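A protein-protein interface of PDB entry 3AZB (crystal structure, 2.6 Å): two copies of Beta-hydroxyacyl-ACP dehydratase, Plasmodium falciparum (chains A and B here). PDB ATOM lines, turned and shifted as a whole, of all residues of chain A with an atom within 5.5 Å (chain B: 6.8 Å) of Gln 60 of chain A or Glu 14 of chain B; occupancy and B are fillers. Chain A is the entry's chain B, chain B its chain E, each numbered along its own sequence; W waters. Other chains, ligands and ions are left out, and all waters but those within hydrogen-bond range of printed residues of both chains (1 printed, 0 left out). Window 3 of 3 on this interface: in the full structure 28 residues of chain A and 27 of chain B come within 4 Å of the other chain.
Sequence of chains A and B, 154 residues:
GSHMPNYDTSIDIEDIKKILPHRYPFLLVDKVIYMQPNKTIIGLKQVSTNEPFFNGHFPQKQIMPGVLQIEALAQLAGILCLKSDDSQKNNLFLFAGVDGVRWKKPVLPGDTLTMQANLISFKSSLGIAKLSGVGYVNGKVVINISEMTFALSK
No position is printed for both chains.
Gln 60 of chain A touches one residue of chain B.
Printed residues of chain B within 4 Å of Lys 61 of chain A: Glu 14 (3.6 Å).
Of the printed residues of chain B, Gln 62 of chain A touches Ile 13, Glu 14 and Lys 17.
Ile 11 of chain B touches none of the printed residues of chain A.
Of the printed residues of chain A, Ile 13 of chain B touches Gln 62 (3.4 Å).
Glu 14 of chain B touches three residues of chain A.
Printed residues of chain A within 4 Å of Lys 17 of chain B: Pro 59 (3.9 Å) and Gln 62 (3.4 Å).
Asp 30 of chain B touches none of the printed residues of chain A.
The nearest printed residue of chain B that does not touch Gln 62 of chain A is Asp 30 of chain B (6.4 Å).
The backbone carbonyl oxygen of Gln 60 of chain A sits close to the side-chain carboxylate of Glu 14 of chain B.
OE2 of Glu 14 of chain B lies within hydrogen-bond range of N of Gln 62 of chain A.
NE2 of Gln 62 of chain A sits close to NZ of Lys 17 of chain B (3.4 Å).
N of Glu 14 of chain B lies within hydrogen-bond range of OD1 of Asp 12 of chain B (3.3 Å).
Water W1 lies within hydrogen-bond range of the side-chain carboxylate of Glu 14 of chain B (3.0 Å) and the backbone carbonyl oxygen of Gln 62 of chain A (3.1 Å).
Among the printed residues, pairs that only touch across the chains: Pro 59 of chain A with Lys 17 of chain B, Lys 61 of chain A with Glu 14 of chain B and Gln 62 of chain A with Ile 13 of chain B.
Along chain A the printed residues that touch a printed residue of chain B span positions 59 to 62.
Printed residues of chain B that touch a printed residue of chain A: Ile 13, Glu 14 and Lys 17.
Hydrophobic or aromatic side chains of chain B within 4 Å of the printed part of chain A: Ile 13.
Among the printed residues, 6 pairs touch across the chains.
Among the printed residues, no Asp or Glu carboxylate lies within 4 Å of a Lys or Arg side-chain nitrogen of the other chain.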
ATOM      1  N   PHE A  58      23.848  23.196 -23.228  1.00  0.00           N
ATOM      2  CA  PHE A  58      24.755  24.207 -22.685  1.00  0.00           C
ATOM      3  C   PHE A  58      24.010  25.541 -22.538  1.00  0.00           C
ATOM      4  O   PHE A  58      22.942  25.725 -23.129  1.00  0.00           O
ATOM      5  CB  PHE A  58      25.961  24.383 -23.613  1.00  0.00           C
ATOM      6  CG  PHE A  58      26.704  23.098 -23.912  1.00  0.00           C
ATOM      7  CD1 PHE A  58      27.667  22.609 -23.027  1.00  0.00           C
ATOM      8  CD2 PHE A  58      26.474  22.398 -25.095  1.00  0.00           C
ATOM      9  CE1 PHE A  58      28.373  21.443 -23.307  1.00  0.00           C
ATOM     10  CE2 PHE A  58      27.180  21.201 -25.373  1.00  0.00           C
ATOM     11  CZ  PHE A  58      28.124  20.737 -24.477  1.00  0.00           C
ATOM     12  N   PRO A  59      24.554  26.471 -21.729  1.00  0.00           N
ATOM     13  CA  PRO A  59      23.922  27.786 -21.627  1.00  0.00           C
ATOM     14  C   PRO A  59      23.623  28.423 -22.990  1.00  0.00           C
ATOM     15  O   PRO A  59      22.501  28.907 -23.223  1.00  0.00           O
ATOM     16  CB  PRO A  59      24.960  28.603 -20.855  1.00  0.00           C
ATOM     17  CG  PRO A  59      25.589  27.619 -19.964  1.00  0.00           C
ATOM     18  CD  PRO A  59      25.535  26.268 -20.648  1.00  0.00           C
ATOM     19  N   GLN A  60      24.615  28.399 -23.876  1.00  0.00           N
ATOM     20  CA  GLN A  60      24.511  29.056 -25.183  1.00  0.00           C
ATOM     21  C   GLN A  60      23.972  28.137 -26.273  1.00  0.00           C
ATOM     22  O   GLN A  60      23.545  28.611 -27.328  1.00  0.00           O
ATOM     23  CB  GLN A  60      25.863  29.660 -25.604  1.00  0.00           C
ATOM     24  CG  GLN A  60      25.892  31.188 -25.631  1.00  0.00           C
ATOM     25  CD  GLN A  60      26.588  31.832 -24.429  1.00  0.00           C
ATOM     26  OE1 GLN A  60      26.049  32.771 -23.815  1.00  0.00           O
ATOM     27  NE2 GLN A  60      27.807  31.352 -24.111  1.00  0.00           N
ATOM     28  N   LYS A  61      23.987  26.830 -26.020  1.00  0.00           N
ATOM     29  CA  LYS A  61      23.420  25.864 -26.956  1.00  0.00           C
ATOM     30  C   LYS A  61      22.806  24.644 -26.250  1.00  0.00           C
ATOM     31  O   LYS A  61      23.522  23.805 -25.694  1.00  0.00           O
ATOM     32  CB  LYS A  61      24.477  25.438 -27.989  1.00  0.00           C
ATOM     33  CG  LYS A  61      23.905  24.865 -29.289  1.00  0.00           C
ATOM     34  CD  LYS A  61      25.015  24.659 -30.318  1.00  0.00           C
ATOM     35  CE  LYS A  61      24.451  24.548 -31.732  1.00  0.00           C
ATOM     36  NZ  LYS A  61      25.537  24.253 -32.722  1.00  0.00           N
ATOM     37  N   GLN A  62      21.478  24.544 -26.297  1.00  0.00           N
ATOM     38  CA  GLN A  62      20.768  23.429 -25.681  1.00  0.00           C
ATOM     39  C   GLN A  62      20.818  22.156 -26.525  1.00  0.00           C
ATOM     40  O   GLN A  62      20.196  22.083 -27.577  1.00  0.00           O
ATOM     41  CB  GLN A  62      19.320  23.828 -25.391  1.00  0.00           C
ATOM     42  CG  GLN A  62      19.190  25.054 -24.494  1.00  0.00           C
ATOM     43  CD  GLN A  62      17.831  25.142 -23.834  1.00  0.00           C
ATOM     44  OE1 GLN A  62      16.827  24.709 -24.403  1.00  0.00           O
ATOM     45  NE2 GLN A  62      17.791  25.704 -22.619  1.00  0.00           N
ATOM     46  N   ILE B  11      11.856  28.878 -36.055  1.00  0.00           N
ATOM     47  CA  ILE B  11      12.615  29.495 -34.977  1.00  0.00           C
ATOM     48  C   ILE B  11      12.864  28.453 -33.875  1.00  0.00           C
ATOM     49  O   ILE B  11      11.973  28.140 -33.086  1.00  0.00           O
ATOM     50  CB  ILE B  11      11.904  30.747 -34.401  1.00  0.00           C
ATOM     51  CG1 ILE B  11      11.485  31.700 -35.532  1.00  0.00           C
ATOM     52  CG2 ILE B  11      12.808  31.446 -33.379  1.00  0.00           C
ATOM     53  CD1 ILE B  11      10.453  32.734 -35.131  1.00  0.00           C
ATOM     54  N   ASP B  12      14.085  27.920 -33.844  1.00  0.00           N
ATOM     55  CA  ASP B  12      14.499  26.964 -32.821  1.00  0.00           C
ATOM     56  C   ASP B  12      14.553  27.639 -31.451  1.00  0.00           C
ATOM     57  O   ASP B  12      14.303  28.842 -31.328  1.00  0.00           O
ATOM     58  CB  ASP B  12      15.867  26.354 -33.163  1.00  0.00           C
ATOM     59  CG  ASP B  12      17.027  27.241 -32.733  1.00  0.00           C
ATOM     60  OD1 ASP B  12      17.922  26.754 -31.995  1.00  0.00           O
ATOM     61  OD2 ASP B  12      17.027  28.434 -33.113  1.00  0.00           O
ATOM     62  N   ILE B  13      14.887  26.850 -30.430  1.00  0.00           N
ATOM     63  CA  ILE B  13      14.910  27.314 -29.035  1.00  0.00           C
ATOM     64  C   ILE B  13      15.899  28.465 -28.737  1.00  0.00           C
ATOM     65  O   ILE B  13      15.510  29.438 -28.103  1.00  0.00           O
ATOM     66  CB  ILE B  13      15.085  26.110 -28.049  1.00  0.00           C
ATOM     67  CG1 ILE B  13      14.911  26.553 -26.594  1.00  0.00           C
ATOM     68  CG2 ILE B  13      16.411  25.390 -28.287  1.00  0.00           C
ATOM     69  CD1 ILE B  13      13.479  26.896 -26.221  1.00  0.00           C
ATOM     70  N   GLU B  14      17.144  28.384 -29.212  1.00  0.00           N
ATOM     71  CA  GLU B  14      18.125  29.460 -28.943  1.00  0.00           C
ATOM     72  C   GLU B  14      17.554  30.825 -29.351  1.00  0.00           C
ATOM     73  O   GLU B  14      17.711  31.814 -28.633  1.00  0.00           O
ATOM     74  CB  GLU B  14      19.481  29.224 -29.633  1.00  0.00           C
ATOM     75  CG  GLU B  14      20.145  27.858 -29.415  1.00  0.00           C
ATOM     76  CD  GLU B  14      20.200  27.412 -27.954  1.00  0.00           C
ATOM     77  OE1 GLU B  14      20.571  28.211 -27.063  1.00  0.00           O
ATOM     78  OE2 GLU B  14      19.880  26.234 -27.701  1.00  0.00           O
ATOM     79  N   ASP B  15      16.867  30.857 -30.494  1.00  0.00           N
ATOM     80  CA  ASP B  15      16.220  32.075 -30.988  1.00  0.00           C
ATOM     81  C   ASP B  15      14.930  32.461 -30.251  1.00  0.00           C
ATOM     82  O   ASP B  15      14.615  33.654 -30.148  1.00  0.00           O
ATOM     83  CB  ASP B  15      15.977  31.974 -32.487  1.00  0.00           C
ATOM     84  CG  ASP B  15      17.241  31.724 -33.255  1.00  0.00           C
ATOM     85  OD1 ASP B  15      18.287  32.301 -32.871  1.00  0.00           O
ATOM     86  OD2 ASP B  15      17.199  30.952 -34.239  1.00  0.00           O
ATOM     87  N   ILE B  16      14.196  31.462 -29.752  1.00  0.00           N
ATOM     88  CA  ILE B  16      13.076  31.681 -28.815  1.00  0.00           C
ATOM     89  C   ILE B  16      13.505  32.435 -27.536  1.00  0.00           C
ATOM     90  O   ILE B  16      12.807  33.363 -27.076  1.00  0.00           O
ATOM     91  CB  ILE B  16      12.374  30.346 -28.433  1.00  0.00           C
ATOM     92  CG1 ILE B  16      11.593  29.784 -29.631  1.00  0.00           C
ATOM     93  CG2 ILE B  16      11.456  30.532 -27.222  1.00  0.00           C
ATOM     94  CD1 ILE B  16      10.912  28.463 -29.388  1.00  0.00           C
ATOM     95  N   LYS B  17      14.650  32.049 -26.975  1.00  0.00           N
ATOM     96  CA  LYS B  17      15.181  32.709 -25.774  1.00  0.00           C
ATOM     97  C   LYS B  17      15.700  34.127 -26.024  1.00  0.00           C
ATOM     98  O   LYS B  17      15.929  34.879 -25.082  1.00  0.00           O
ATOM     99  CB  LYS B  17      16.278  31.859 -25.132  1.00  0.00           C
ATOM    100  CG  LYS B  17      15.734  30.739 -24.277  1.00  0.00           C
ATOM    101  CD  LYS B  17      16.807  29.702 -23.952  1.00  0.00           C
ATOM    102  CE  LYS B  17      17.727  30.114 -22.800  1.00  0.00           C
ATOM    103  NZ  LYS B  17      18.645  28.970 -22.504  1.00  0.00           N
ATOM    104  N   LYS B  18      15.882  34.480 -27.292  1.00  0.00           N
ATOM    105  CA  LYS B  18      16.279  35.830 -27.674  1.00  0.00           C
ATOM    106  C   LYS B  18      15.050  36.725 -27.787  1.00  0.00           C
ATOM    107  O   LYS B  18      15.151  37.946 -27.748  1.00  0.00           O
ATOM    108  CB  LYS B  18      17.023  35.811 -29.014  1.00  0.00           C
ATOM    109  CG  LYS B  18      18.391  35.137 -28.983  1.00  0.00           C
ATOM    110  CD  LYS B  18      18.988  35.069 -30.391  1.00  0.00           C
ATOM    111  CE  LYS B  18      20.496  34.867 -30.312  1.00  0.00           C
ATOM    112  NZ  LYS B  18      21.094  34.504 -31.651  1.00  0.00           N
ATOM    113  N   ILE B  19      13.890  36.105 -27.945  1.00  0.00           N
ATOM    114  CA  ILE B  19      12.638  36.848 -28.046  1.00  0.00           C
ATOM    115  C   ILE B  19      11.997  36.945 -26.668  1.00  0.00           C
ATOM    116  O   ILE B  19      11.735  38.042 -26.188  1.00  0.00           O
ATOM    117  CB  ILE B  19      11.667  36.215 -29.098  1.00  0.00           C
ATOM    118  CG1 ILE B  19      12.296  36.284 -30.495  1.00  0.00           C
ATOM    119  CG2 ILE B  19      10.309  36.909 -29.077  1.00  0.00           C
ATOM    120  CD1 ILE B  19      11.906  35.157 -31.420  1.00  0.00           C
ATOM    121  N   ASP B  30       8.943  24.767 -26.826  1.00  0.00           N
ATOM    122  CA  ASP B  30      10.139  24.064 -27.271  1.00  0.00           C
ATOM    123  C   ASP B  30      10.598  24.452 -28.675  1.00  0.00           C
ATOM    124  O   ASP B  30      11.797  24.577 -28.910  1.00  0.00           O
ATOM    125  CB  ASP B  30       9.946  22.560 -27.143  1.00  0.00           C
ATOM    126  CG  ASP B  30      10.040  22.086 -25.708  1.00  0.00           C
ATOM    127  OD1 ASP B  30      10.814  22.660 -24.935  1.00  0.00           O
ATOM    128  OD2 ASP B  30       9.354  21.126 -25.340  1.00  0.00           O
HETATM  129  O   HOH W   1      19.749  24.125 -29.893  1.00  0.00           O
